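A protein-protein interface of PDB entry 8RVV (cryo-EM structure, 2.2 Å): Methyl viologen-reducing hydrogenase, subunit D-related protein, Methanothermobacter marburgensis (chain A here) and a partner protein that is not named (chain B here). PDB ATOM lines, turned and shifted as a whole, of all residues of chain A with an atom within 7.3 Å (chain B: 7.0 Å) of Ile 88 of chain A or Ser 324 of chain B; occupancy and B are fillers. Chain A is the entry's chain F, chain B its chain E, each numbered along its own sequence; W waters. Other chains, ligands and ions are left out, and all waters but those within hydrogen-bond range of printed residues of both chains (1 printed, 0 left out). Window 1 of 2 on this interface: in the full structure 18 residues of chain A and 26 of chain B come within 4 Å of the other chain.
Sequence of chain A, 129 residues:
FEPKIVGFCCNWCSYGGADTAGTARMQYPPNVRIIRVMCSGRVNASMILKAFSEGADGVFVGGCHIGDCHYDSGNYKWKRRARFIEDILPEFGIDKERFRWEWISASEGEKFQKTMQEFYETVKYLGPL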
ATOM      1  N   ASN A  44      12.022   8.650 -18.116  1.00  0.00           N
ATOM      2  CA  ASN A  44      10.609   8.305 -18.129  1.00  0.00           C
ATOM      3  C   ASN A  44      10.464   6.789 -18.163  1.00  0.00           C
ATOM      4  O   ASN A  44      11.437   6.049 -18.319  1.00  0.00           O
ATOM      5  CB  ASN A  44       9.871   8.954 -19.312  1.00  0.00           C
ATOM      6  CG  ASN A  44      10.362   8.463 -20.660  1.00  0.00           C
ATOM      7  OD1 ASN A  44      11.189   7.562 -20.749  1.00  0.00           O
ATOM      8  ND2 ASN A  44       9.847   9.063 -21.721  1.00  0.00           N
ATOM      9  N   ALA A  45       9.223   6.331 -18.009  1.00  0.00           N
ATOM     10  CA  ALA A  45       8.949   4.905 -17.887  1.00  0.00           C
ATOM     11  C   ALA A  45       9.303   4.121 -19.140  1.00  0.00           C
ATOM     12  O   ALA A  45       9.555   2.918 -19.045  1.00  0.00           O
ATOM     13  CB  ALA A  45       7.479   4.686 -17.562  1.00  0.00           C
ATOM     14  N   SER A  46       9.315   4.762 -20.310  1.00  0.00           N
ATOM     15  CA  SER A  46       9.658   4.039 -21.528  1.00  0.00           C
ATOM     16  C   SER A  46      11.071   3.485 -21.453  1.00  0.00           C
ATOM     17  O   SER A  46      11.324   2.364 -21.902  1.00  0.00           O
ATOM     18  CB  SER A  46       9.504   4.943 -22.749  1.00  0.00           C
ATOM     19  OG  SER A  46       8.142   5.098 -23.098  1.00  0.00           O
ATOM     20  N   LEU A  49      11.058   0.434 -19.036  1.00  0.00           N
ATOM     21  CA  LEU A  49      10.392  -0.703 -19.659  1.00  0.00           C
ATOM     22  C   LEU A  49      11.223  -1.273 -20.797  1.00  0.00           C
ATOM     23  O   LEU A  49      11.288  -2.493 -20.973  1.00  0.00           O
ATOM     24  CB  LEU A  49       9.008  -0.289 -20.152  1.00  0.00           C
ATOM     25  CG  LEU A  49       8.007  -0.003 -19.037  1.00  0.00           C
ATOM     26  CD1 LEU A  49       6.882   0.878 -19.535  1.00  0.00           C
ATOM     27  CD2 LEU A  49       7.467  -1.299 -18.464  1.00  0.00           C
ATOM     28  N   ARG A  81       7.170   9.985 -11.609  1.00  0.00           N
ATOM     29  CA  ARG A  81       7.236   8.939 -12.623  1.00  0.00           C
ATOM     30  C   ARG A  81       7.654   7.610 -12.012  1.00  0.00           C
ATOM     31  O   ARG A  81       7.147   6.555 -12.402  1.00  0.00           O
ATOM     32  CB  ARG A  81       8.210   9.342 -13.726  1.00  0.00           C
ATOM     33  CG  ARG A  81       7.668  10.373 -14.688  1.00  0.00           C
ATOM     34  CD  ARG A  81       8.751  10.886 -15.612  1.00  0.00           C
ATOM     35  NE  ARG A  81       8.497  12.249 -16.063  1.00  0.00           N
ATOM     36  CZ  ARG A  81       9.437  13.087 -16.475  1.00  0.00           C
ATOM     37  NH1 ARG A  81      10.710  12.736 -16.504  1.00  0.00           N
ATOM     38  NH2 ARG A  81       9.090  14.307 -16.874  1.00  0.00           N
ATOM     39  N   ALA A  82       8.588   7.645 -11.063  1.00  0.00           N
ATOM     40  CA  ALA A  82       9.136   6.430 -10.474  1.00  0.00           C
ATOM     41  C   ALA A  82       8.096   5.711  -9.635  1.00  0.00           C
ATOM     42  O   ALA A  82       8.015   4.478  -9.659  1.00  0.00           O
ATOM     43  CB  ALA A  82      10.351   6.772  -9.617  1.00  0.00           C
ATOM     44  N   ARG A  83       7.308   6.466  -8.870  1.00  0.00           N
ATOM     45  CA  ARG A  83       6.205   5.855  -8.137  1.00  0.00           C
ATOM     46  C   ARG A  83       5.230   5.182  -9.095  1.00  0.00           C
ATOM     47  O   ARG A  83       4.814   4.035  -8.871  1.00  0.00           O
ATOM     48  CB  ARG A  83       5.514   6.923  -7.295  1.00  0.00           C
ATOM     49  CG  ARG A  83       6.071   7.095  -5.886  1.00  0.00           C
ATOM     50  CD  ARG A  83       6.108   5.856  -4.936  1.00  0.00           C
ATOM     51  NE  ARG A  83       4.826   5.172  -4.772  1.00  0.00           N
ATOM     52  CZ  ARG A  83       4.375   4.157  -5.495  1.00  0.00           C
ATOM     53  NH1 ARG A  83       5.141   3.526  -6.360  1.00  0.00           N
ATOM     54  NH2 ARG A  83       3.127   3.741  -5.319  1.00  0.00           N
ATOM     55  N   PHE A  84       4.883   5.860 -10.196  1.00  0.00           N
ATOM     56  CA  PHE A  84       3.969   5.240 -11.154  1.00  0.00           C
ATOM     57  C   PHE A  84       4.583   3.983 -11.771  1.00  0.00           C
ATOM     58  O   PHE A  84       3.885   2.989 -12.010  1.00  0.00           O
ATOM     59  CB  PHE A  84       3.582   6.245 -12.240  1.00  0.00           C
ATOM     60  CG  PHE A  84       2.407   5.825 -13.079  1.00  0.00           C
ATOM     61  CD1 PHE A  84       1.327   5.182 -12.506  1.00  0.00           C
ATOM     62  CD2 PHE A  84       2.375   6.085 -14.436  1.00  0.00           C
ATOM     63  CE1 PHE A  84       0.249   4.805 -13.263  1.00  0.00           C
ATOM     64  CE2 PHE A  84       1.292   5.707 -15.200  1.00  0.00           C
ATOM     65  CZ  PHE A  84       0.228   5.065 -14.610  1.00  0.00           C
ATOM     66  N   ILE A  85       5.884   4.009 -12.049  1.00  0.00           N
ATOM     67  CA  ILE A  85       6.548   2.846 -12.628  1.00  0.00           C
ATOM     68  C   ILE A  85       6.540   1.677 -11.648  1.00  0.00           C
ATOM     69  O   ILE A  85       6.370   0.519 -12.044  1.00  0.00           O
ATOM     70  CB  ILE A  85       7.980   3.208 -13.057  1.00  0.00           C
ATOM     71  CG1 ILE A  85       7.965   4.160 -14.255  1.00  0.00           C
ATOM     72  CG2 ILE A  85       8.763   1.959 -13.395  1.00  0.00           C
ATOM     73  CD1 ILE A  85       9.209   5.015 -14.362  1.00  0.00           C
ATOM     74  N   GLU A  86       6.781   1.948 -10.363  1.00  0.00           N
ATOM     75  CA  GLU A  86       6.657   0.892  -9.365  1.00  0.00           C
ATOM     76  C   GLU A  86       5.246   0.329  -9.341  1.00  0.00           C
ATOM     77  O   GLU A  86       5.058  -0.864  -9.094  1.00  0.00           O
ATOM     78  CB  GLU A  86       7.030   1.408  -7.978  1.00  0.00           C
ATOM     79  CG  GLU A  86       8.489   1.742  -7.799  1.00  0.00           C
ATOM     80  CD  GLU A  86       8.759   2.484  -6.507  1.00  0.00           C
ATOM     81  OE1 GLU A  86       9.915   2.461  -6.037  1.00  0.00           O
ATOM     82  OE2 GLU A  86       7.820   3.099  -5.967  1.00  0.00           O
ATOM     83  N   ASP A  87       4.243   1.174  -9.580  1.00  0.00           N
ATOM     84  CA  ASP A  87       2.887   0.653  -9.723  1.00  0.00           C
ATOM     85  C   ASP A  87       2.780  -0.286 -10.922  1.00  0.00           C
ATOM     86  O   ASP A  87       2.174  -1.357 -10.831  1.00  0.00           O
ATOM     87  CB  ASP A  87       1.885   1.801  -9.856  1.00  0.00           C
ATOM     88  CG  ASP A  87       1.461   2.370  -8.515  1.00  0.00           C
ATOM     89  OD1 ASP A  87       1.542   1.643  -7.504  1.00  0.00           O
ATOM     90  OD2 ASP A  87       1.042   3.545  -8.471  1.00  0.00           O
ATOM     91  N   ILE A  88       3.385   0.090 -12.048  1.00  0.00           N
ATOM     92  CA  ILE A  88       3.124  -0.621 -13.300  1.00  0.00           C
ATOM     93  C   ILE A  88       3.900  -1.935 -13.371  1.00  0.00           C
ATOM     94  O   ILE A  88       3.398  -2.934 -13.895  1.00  0.00           O
ATOM     95  CB  ILE A  88       3.445   0.290 -14.499  1.00  0.00           C
ATOM     96  CG1 ILE A  88       2.314   1.297 -14.708  1.00  0.00           C
ATOM     97  CG2 ILE A  88       3.659  -0.533 -15.758  1.00  0.00           C
ATOM     98  CD1 ILE A  88       2.688   2.470 -15.580  1.00  0.00           C
ATOM     99  N   LEU A  89       5.134  -1.958 -12.866  1.00  0.00           N
ATOM    100  CA  LEU A  89       6.022  -3.092 -13.133  1.00  0.00           C
ATOM    101  C   LEU A  89       5.494  -4.421 -12.605  1.00  0.00           C
ATOM    102  O   LEU A  89       5.563  -5.421 -13.339  1.00  0.00           O
ATOM    103  CB  LEU A  89       7.417  -2.801 -12.570  1.00  0.00           C
ATOM    104  CG  LEU A  89       8.256  -1.801 -13.364  1.00  0.00           C
ATOM    105  CD1 LEU A  89       9.419  -1.311 -12.520  1.00  0.00           C
ATOM    106  CD2 LEU A  89       8.749  -2.403 -14.666  1.00  0.00           C
ATOM    107  N   PRO A  90       4.987  -4.523 -11.375  1.00  0.00           N
ATOM    108  CA  PRO A  90       4.542  -5.837 -10.879  1.00  0.00           C
ATOM    109  C   PRO A  90       3.422  -6.460 -11.695  1.00  0.00           C
ATOM    110  O   PRO A  90       3.230  -7.679 -11.620  1.00  0.00           O
ATOM    111  CB  PRO A  90       4.087  -5.535  -9.447  1.00  0.00           C
ATOM    112  CG  PRO A  90       4.776  -4.277  -9.080  1.00  0.00           C
ATOM    113  CD  PRO A  90       4.882  -3.487 -10.338  1.00  0.00           C
ATOM    114  N   GLU A  91       2.673  -5.670 -12.467  1.00  0.00           N
ATOM    115  CA  GLU A  91       1.593  -6.209 -13.285  1.00  0.00           C
ATOM    116  C   GLU A  91       2.091  -7.096 -14.413  1.00  0.00           C
ATOM    117  O   GLU A  91       1.289  -7.835 -14.994  1.00  0.00           O
ATOM    118  CB  GLU A  91       0.761  -5.074 -13.875  1.00  0.00           C
ATOM    119  CG  GLU A  91       0.177  -4.147 -12.838  1.00  0.00           C
ATOM    120  CD  GLU A  91      -1.136  -4.644 -12.280  1.00  0.00           C
ATOM    121  OE1 GLU A  91      -1.248  -5.855 -12.005  1.00  0.00           O
ATOM    122  OE2 GLU A  91      -2.060  -3.821 -12.118  1.00  0.00           O
ATOM    123  N   PHE A  92       3.380  -7.047 -14.735  1.00  0.00           N
ATOM    124  CA  PHE A  92       3.953  -7.876 -15.785  1.00  0.00           C
ATOM    125  C   PHE A  92       5.006  -8.834 -15.240  1.00  0.00           C
ATOM    126  O   PHE A  92       5.890  -9.267 -15.982  1.00  0.00           O
ATOM    127  CB  PHE A  92       4.530  -6.986 -16.885  1.00  0.00           C
ATOM    128  CG  PHE A  92       3.504  -6.103 -17.523  1.00  0.00           C
ATOM    129  CD1 PHE A  92       3.222  -4.857 -16.997  1.00  0.00           C
ATOM    130  CD2 PHE A  92       2.796  -6.531 -18.634  1.00  0.00           C
ATOM    131  CE1 PHE A  92       2.268  -4.052 -17.571  1.00  0.00           C
ATOM    132  CE2 PHE A  92       1.841  -5.728 -19.214  1.00  0.00           C
ATOM    133  CZ  PHE A  92       1.578  -4.486 -18.683  1.00  0.00           C
ATOM    134  N   GLY A  93       4.918  -9.177 -13.958  1.00  0.00           N
ATOM    135  CA  GLY A  93       5.816 -10.151 -13.373  1.00  0.00           C
ATOM    136  C   GLY A  93       7.203  -9.646 -13.056  1.00  0.00           C
ATOM    137  O   GLY A  93       8.125 -10.456 -12.934  1.00  0.00           O
ATOM    138  N   ILE A  94       7.384  -8.339 -12.915  1.00  0.00           N
ATOM    139  CA  ILE A  94       8.667  -7.746 -12.547  1.00  0.00           C
ATOM    140  C   ILE A  94       8.525  -7.217 -11.127  1.00  0.00           C
ATOM    141  O   ILE A  94       7.746  -6.291 -10.873  1.00  0.00           O
ATOM    142  CB  ILE A  94       9.085  -6.638 -13.523  1.00  0.00           C
ATOM    143  CG1 ILE A  94       9.125  -7.182 -14.952  1.00  0.00           C
ATOM    144  CG2 ILE A  94      10.441  -6.058 -13.136  1.00  0.00           C
ATOM    145  CD1 ILE A  94       9.570  -6.179 -15.985  1.00  0.00           C
ATOM    146  N   LEU B 316       5.378  -5.601 -22.372  1.00  0.00           N
ATOM    147  CA  LEU B 316       6.043  -4.462 -21.760  1.00  0.00           C
ATOM    148  C   LEU B 316       6.038  -3.284 -22.724  1.00  0.00           C
ATOM    149  O   LEU B 316       5.301  -2.320 -22.512  1.00  0.00           O
ATOM    150  CB  LEU B 316       7.474  -4.820 -21.355  1.00  0.00           C
ATOM    151  CG  LEU B 316       7.622  -5.595 -20.046  1.00  0.00           C
ATOM    152  CD1 LEU B 316       9.029  -6.153 -19.924  1.00  0.00           C
ATOM    153  CD2 LEU B 316       7.289  -4.724 -18.852  1.00  0.00           C
ATOM    154  N   GLN B 319       1.950  -2.491 -23.865  1.00  0.00           N
ATOM    155  CA  GLN B 319       0.967  -2.192 -22.834  1.00  0.00           C
ATOM    156  C   GLN B 319       1.567  -1.343 -21.725  1.00  0.00           C
ATOM    157  O   GLN B 319       0.934  -0.390 -21.270  1.00  0.00           O
ATOM    158  CB  GLN B 319       0.387  -3.486 -22.261  1.00  0.00           C
ATOM    159  CG  GLN B 319      -0.168  -4.445 -23.298  1.00  0.00           C
ATOM    160  CD  GLN B 319      -1.462  -3.962 -23.924  1.00  0.00           C
ATOM    161  OE1 GLN B 319      -2.140  -3.089 -23.385  1.00  0.00           O
ATOM    162  NE2 GLN B 319      -1.806  -4.525 -25.071  1.00  0.00           N
ATOM    163  N   GLY B 320       2.771  -1.681 -21.252  1.00  0.00           N
ATOM    164  CA  GLY B 320       3.371  -0.893 -20.195  1.00  0.00           C
ATOM    165  C   GLY B 320       3.699   0.513 -20.641  1.00  0.00           C
ATOM    166  O   GLY B 320       3.577   1.456 -19.860  1.00  0.00           O
ATOM    167  N   VAL B 321       4.109   0.680 -21.896  1.00  0.00           N
ATOM    168  CA  VAL B 321       4.365   2.019 -22.411  1.00  0.00           C
ATOM    169  C   VAL B 321       3.071   2.822 -22.464  1.00  0.00           C
ATOM    170  O   VAL B 321       3.021   3.971 -22.012  1.00  0.00           O
ATOM    171  CB  VAL B 321       5.050   1.947 -23.786  1.00  0.00           C
ATOM    172  CG1 VAL B 321       5.173   3.337 -24.389  1.00  0.00           C
ATOM    173  CG2 VAL B 321       6.414   1.305 -23.659  1.00  0.00           C
ATOM    174  N   ARG B 322       1.999   2.233 -23.005  1.00  0.00           N
ATOM    175  CA  ARG B 322       0.734   2.963 -23.039  1.00  0.00           C
ATOM    176  C   ARG B 322       0.244   3.276 -21.627  1.00  0.00           C
ATOM    177  O   ARG B 322      -0.319   4.351 -21.379  1.00  0.00           O
ATOM    178  CB  ARG B 322      -0.315   2.169 -23.817  1.00  0.00           C
ATOM    179  CG  ARG B 322      -1.575   2.959 -24.133  1.00  0.00           C
ATOM    180  CD  ARG B 322      -2.365   2.354 -25.287  1.00  0.00           C
ATOM    181  NE  ARG B 322      -3.451   1.499 -24.824  1.00  0.00           N
ATOM    182  CZ  ARG B 322      -4.590   1.942 -24.308  1.00  0.00           C
ATOM    183  NH1 ARG B 322      -4.847   3.232 -24.204  1.00  0.00           N
ATOM    184  NH2 ARG B 322      -5.491   1.063 -23.885  1.00  0.00           N
ATOM    185  N   LEU B 323       0.443   2.345 -20.691  1.00  0.00           N
ATOM    186  CA  LEU B 323       0.071   2.581 -19.300  1.00  0.00           C
ATOM    187  C   LEU B 323       0.842   3.759 -18.723  1.00  0.00           C
ATOM    188  O   LEU B 323       0.249   4.681 -18.170  1.00  0.00           O
ATOM    189  CB  LEU B 323       0.319   1.324 -18.470  1.00  0.00           C
ATOM    190  CG  LEU B 323      -0.732   0.220 -18.565  1.00  0.00           C
ATOM    191  CD1 LEU B 323      -0.140  -1.096 -18.112  1.00  0.00           C
ATOM    192  CD2 LEU B 323      -1.960   0.566 -17.741  1.00  0.00           C
ATOM    193  N   SER B 324       2.159   3.770 -18.886  1.00  0.00           N
ATOM    194  CA  SER B 324       2.931   4.905 -18.403  1.00  0.00           C
ATOM    195  C   SER B 324       2.492   6.204 -19.065  1.00  0.00           C
ATOM    196  O   SER B 324       2.576   7.272 -18.451  1.00  0.00           O
ATOM    197  CB  SER B 324       4.413   4.665 -18.647  1.00  0.00           C
ATOM    198  OG  SER B 324       4.761   4.936 -19.990  1.00  0.00           O
ATOM    199  N   HIS B 325       2.024   6.135 -20.313  1.00  0.00           N
ATOM    200  CA  HIS B 325       1.641   7.353 -21.023  1.00  0.00           C
ATOM    201  C   HIS B 325       0.327   7.925 -20.506  1.00  0.00           C
ATOM    202  O   HIS B 325       0.203   9.143 -20.351  1.00  0.00           O
ATOM    203  CB  HIS B 325       1.526   7.076 -22.520  1.00  0.00           C
ATOM    204  CG  HIS B 325       2.821   7.191 -23.258  1.00  0.00           C
ATOM    205  ND1 HIS B 325       2.891   7.176 -24.635  1.00  0.00           N
ATOM    206  CD2 HIS B 325       4.094   7.315 -22.819  1.00  0.00           C
ATOM    207  CE1 HIS B 325       4.151   7.289 -25.009  1.00  0.00           C
ATOM    208  NE2 HIS B 325       4.902   7.375 -23.927  1.00  0.00           N
ATOM    209  N   MET B 326      -0.676   7.077 -20.268  1.00  0.00           N
ATOM    210  CA  MET B 326      -2.008   7.601 -19.986  1.00  0.00           C
ATOM    211  C   MET B 326      -2.804   6.869 -18.912  1.00  0.00           C
ATOM    212  O   MET B 326      -3.962   7.232 -18.695  1.00  0.00           O
ATOM    213  CB  MET B 326      -2.845   7.628 -21.281  1.00  0.00           C
ATOM    214  CG  MET B 326      -2.759   6.366 -22.133  1.00  0.00           C
ATOM    215  SD  MET B 326      -3.418   4.892 -21.331  1.00  0.00           S
ATOM    216  CE  MET B 326      -5.134   5.334 -21.130  1.00  0.00           C
ATOM    217  N   GLY B 327      -2.242   5.876 -18.224  1.00  0.00           N
ATOM    218  CA  GLY B 327      -3.039   5.053 -17.337  1.00  0.00           C
ATOM    219  C   GLY B 327      -3.530   5.794 -16.116  1.00  0.00           C
ATOM    220  O   GLY B 327      -4.501   5.373 -15.485  1.00  0.00           O
ATOM    221  N   PHE B 328      -2.857   6.883 -15.749  1.00  0.00           N
ATOM    222  CA  PHE B 328      -3.380   7.773 -14.720  1.00  0.00           C
ATOM    223  C   PHE B 328      -4.601   8.544 -15.198  1.00  0.00           C
ATOM    224  O   PHE B 328      -5.348   9.062 -14.366  1.00  0.00           O
ATOM    225  CB  PHE B 328      -2.292   8.749 -14.257  1.00  0.00           C
ATOM    226  CG  PHE B 328      -1.490   9.346 -15.380  1.00  0.00           C
ATOM    227  CD1 PHE B 328      -2.025  10.335 -16.182  1.00  0.00           C
ATOM    228  CD2 PHE B 328      -0.203   8.911 -15.634  1.00  0.00           C
ATOM    229  CE1 PHE B 328      -1.292  10.879 -17.213  1.00  0.00           C
ATOM    230  CE2 PHE B 328       0.532   9.451 -16.664  1.00  0.00           C
ATOM    231  CZ  PHE B 328      -0.012  10.437 -17.453  1.00  0.00           C
ATOM    232  N   ILE B 349      -6.703  -4.248 -16.525  1.00  0.00           N
ATOM    233  CA  ILE B 349      -5.387  -3.822 -16.070  1.00  0.00           C
ATOM    234  C   ILE B 349      -5.294  -2.304 -16.061  1.00  0.00           C
ATOM    235  O   ILE B 349      -4.744  -1.709 -15.125  1.00  0.00           O
ATOM    236  CB  ILE B 349      -4.276  -4.461 -16.927  1.00  0.00           C
ATOM    237  CG1 ILE B 349      -2.915  -3.871 -16.552  1.00  0.00           C
ATOM    238  CG2 ILE B 349      -4.526  -4.260 -18.409  1.00  0.00           C
ATOM    239  CD1 ILE B 349      -1.766  -4.782 -16.841  1.00  0.00           C
ATOM    240  N   TYR B 350      -5.831  -1.646 -17.093  1.00  0.00           N
ATOM    241  CA  TYR B 350      -5.727  -0.188 -17.123  1.00  0.00           C
ATOM    242  C   TYR B 350      -6.486   0.446 -15.958  1.00  0.00           C
ATOM    243  O   TYR B 350      -5.985   1.377 -15.316  1.00  0.00           O
ATOM    244  CB  TYR B 350      -6.208   0.347 -18.470  1.00  0.00           C
ATOM    245  CG  TYR B 350      -5.136   0.248 -19.530  1.00  0.00           C
ATOM    246  CD1 TYR B 350      -4.820  -0.972 -20.104  1.00  0.00           C
ATOM    247  CD2 TYR B 350      -4.416   1.365 -19.932  1.00  0.00           C
ATOM    248  CE1 TYR B 350      -3.834  -1.081 -21.054  1.00  0.00           C
ATOM    249  CE2 TYR B 350      -3.426   1.265 -20.885  1.00  0.00           C
ATOM    250  CZ  TYR B 350      -3.141   0.038 -21.442  1.00  0.00           C
ATOM    251  OH  TYR B 350      -2.163  -0.081 -22.393  1.00  0.00           O
ATOM    252  N   ILE B 353      -4.544  -0.085 -12.635  1.00  0.00           N
ATOM    253  CA  ILE B 353      -3.429   0.851 -12.517  1.00  0.00           C
ATOM    254  C   ILE B 353      -3.937   2.250 -12.179  1.00  0.00           C
ATOM    255  O   ILE B 353      -3.392   2.936 -11.302  1.00  0.00           O
ATOM    256  CB  ILE B 353      -2.594   0.849 -13.809  1.00  0.00           C
ATOM    257  CG1 ILE B 353      -1.749  -0.421 -13.887  1.00  0.00           C
ATOM    258  CG2 ILE B 353      -1.738   2.099 -13.894  1.00  0.00           C
ATOM    259  CD1 ILE B 353      -0.567  -0.439 -12.947  1.00  0.00           C
ATOM    260  N   LYS B 356      -4.773   2.428  -8.558  1.00  0.00           N
ATOM    261  CA  LYS B 356      -3.585   2.613  -7.731  1.00  0.00           C
ATOM    262  C   LYS B 356      -3.161   4.076  -7.715  1.00  0.00           C
ATOM    263  O   LYS B 356      -2.910   4.659  -6.650  1.00  0.00           O
ATOM    264  CB  LYS B 356      -2.441   1.743  -8.243  1.00  0.00           C
ATOM    265  CG  LYS B 356      -2.593   0.259  -7.995  1.00  0.00           C
ATOM    266  CD  LYS B 356      -1.513  -0.499  -8.744  1.00  0.00           C
ATOM    267  CE  LYS B 356      -1.626  -1.995  -8.545  1.00  0.00           C
ATOM    268  NZ  LYS B 356      -0.628  -2.730  -9.369  1.00  0.00           N
ATOM    269  N   MET B 374       1.102  14.145 -12.178  1.00  0.00           N
ATOM    270  CA  MET B 374       2.283  13.826 -12.969  1.00  0.00           C
ATOM    271  C   MET B 374       2.810  15.050 -13.701  1.00  0.00           C
ATOM    272  O   MET B 374       4.023  15.180 -13.898  1.00  0.00           O
ATOM    273  CB  MET B 374       1.949  12.720 -13.971  1.00  0.00           C
ATOM    274  CG  MET B 374       3.157  12.097 -14.652  1.00  0.00           C
ATOM    275  SD  MET B 374       4.249  11.214 -13.525  1.00  0.00           S
ATOM    276  CE  MET B 374       3.192   9.870 -13.001  1.00  0.00           C
ATOM    277  N   TYR B 375       1.921  15.955 -14.110  1.00  0.00           N
ATOM    278  CA  TYR B 375       2.291  17.107 -14.920  1.00  0.00           C
ATOM    279  C   TYR B 375       2.358  18.400 -14.118  1.00  0.00           C
ATOM    280  O   TYR B 375       2.424  19.479 -14.711  1.00  0.00           O
ATOM    281  CB  TYR B 375       1.309  17.260 -16.084  1.00  0.00           C
ATOM    282  CG  TYR B 375       1.315  16.082 -17.028  1.00  0.00           C
ATOM    283  CD1 TYR B 375       2.508  15.545 -17.484  1.00  0.00           C
ATOM    284  CD2 TYR B 375       0.131  15.503 -17.455  1.00  0.00           C
ATOM    285  CE1 TYR B 375       2.524  14.468 -18.338  1.00  0.00           C
ATOM    286  CE2 TYR B 375       0.137  14.426 -18.315  1.00  0.00           C
ATOM    287  CZ  TYR B 375       1.338  13.912 -18.752  1.00  0.00           C
ATOM    288  OH  TYR B 375       1.357  12.841 -19.609  1.00  0.00           O
HETATM  289  O   HOH W   1       7.098   6.811 -21.052  1.00  0.00           O
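Hydrophobic or aromatic side chains of chain B that line the printed part of chain A: Leu 316, Val 321, Leu 323, Phe 328, Ile 349, Ile 353 and Met 374. Along chain B the printed residues that touch a printed residue of chain A span positions 316 to 374. Of the 18 printed residues of chain A, 10 touch a printed residue of chain B. Hydrophobic or aromatic side chains of chain A within 4 Å of the printed part of chain B: Ala 45, Leu 49, Phe 84, Ile 88, Phe 92 and Ile 94. Among the printed residues, 24 pairs touch across the chains. Among the printed residues, Asp or Glu carboxylates within 4 Å of a Lys or Arg side-chain nitrogen of the other chain: Glu 91 of chain A with Lys 356 of chain B (3.3 Å).
O of Leu 89 of chain A sits at hydrogen-bond distance from N of Ile 94 of chain A (3.5 Å). O of Val 321 of chain B is in hydrogen-bond range of OG of Ser 324 of chain B, at 2.8 Å. The side-chain amide oxygen (OE1) of Gln 319 of chain B sits at hydrogen-bond distance from the side-chain hydroxyl (OH) of Tyr 350 of chain B (3.2 Å). The backbone NH of Ser 46 of chain A lies close to the side-chain amide oxygen of Asn 44 of chain A (3.4 Å). The backbone NH (N) of Val 321 of chain B lies within hydrogen-bond range of the backbone carbonyl oxygen (O) of Leu 316 of chain B. NH2 of Arg 83 of chain A is in salt-bridge range of OD1 of Asp 87 of chain A, 3.4 Å away.
Printed residues of chain B within 4 Å of Ile 88 of chain A: Leu 323 (3.9 Å), Ser 324 (3.6 Å) and Ile 353 (3.7 Å). Of chain A, only Ala 45, Phe 84 and Ile 88 come within 4 Å of Ser 324 of chain B. Of the printed residues of chain A, Gln 319 of chain B touches Phe 92 (3.9 Å). Printed residues of chain B within 4 Å of Ala 45 of chain A: Ser 324 (3.3 Å). Of the printed residues of chain A, Ile 353 of chain B touches Phe 84 (3.4 Å), Asp 87 (3.6 Å), Ile 88 (3.7 Å) and Glu 91 (3.8 Å). Of the printed residues of chain B, Arg 81 of chain A touches Met 374 (3.7 Å). Of the printed residues of chain B, Ile 94 of chain A touches Leu 316.
Water W1 lies within hydrogen-bond range of the side-chain hydroxyl (OG) of Ser 46 of chain A (2.9 Å) and the side-chain hydroxyl (OG) of Ser 324 of chain B (3.2 Å).
SD of Met 374 of chain B lies within hydrogen-bond range of N of Arg 81 of chain A (3.7 Å). NZ of Lys 356 of chain B sits at hydrogen-bond distance from O of Asp 87 of chain A (3.4 Å). NZ of Lys 356 of chain B is in salt-bridge range of OE2 of Glu 91 of chain A, 3.3 Å away.
Among the printed residues, merely in contact across the chains: Ala 45 of chain A with Ser 324 of chain B (3.3 Å), Ser 46 of chain A with Val 321 of chain B (3.7 Å), Leu 49 of chain A with Leu 316 of chain B (3.5 Å), Leu 49 of chain A with Gly 320 of chain B (3.4 Å), Leu 49 of chain A with Val 321 of chain B (3.6 Å), Phe 84 of chain A with Leu 323 of chain B (3.3 Å), Phe 84 of chain A with Ser 324 of chain B (3.7 Å), Phe 84 of chain A with Phe 328 of chain B (3.6 Å), Phe 84 of chain A with Ile 353 of chain B (3.4 Å), Phe 84 of chain A with Met 374 of chain B (3.7 Å), Asp 87 of chain A with Ile 353 of chain B (3.6 Å), Ile 88 of chain A with Leu 323 of chain B (3.9 Å), Ile 88 of chain A with Ser 324 of chain B (3.6 Å), Ile 88 of chain A with Ile 353 of chain B (3.7 Å), Glu 91 of chain A with Ile 349 of chain B (3.9 Å), Glu 91 of chain A with Ile 353 of chain B (3.8 Å), Phe 92 of chain A with Gln 319 of chain B (3.9 Å), Phe 92 of chain A with Gly 320 of chain B (3.99 Å), Phe 92 of chain A with Leu 323 of chain B (3.8 Å), Phe 92 of chain A with Ile 349 of chain B (3.8 Å) and Ile 94 of chain A with Leu 316 of chain B (3.9 Å).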
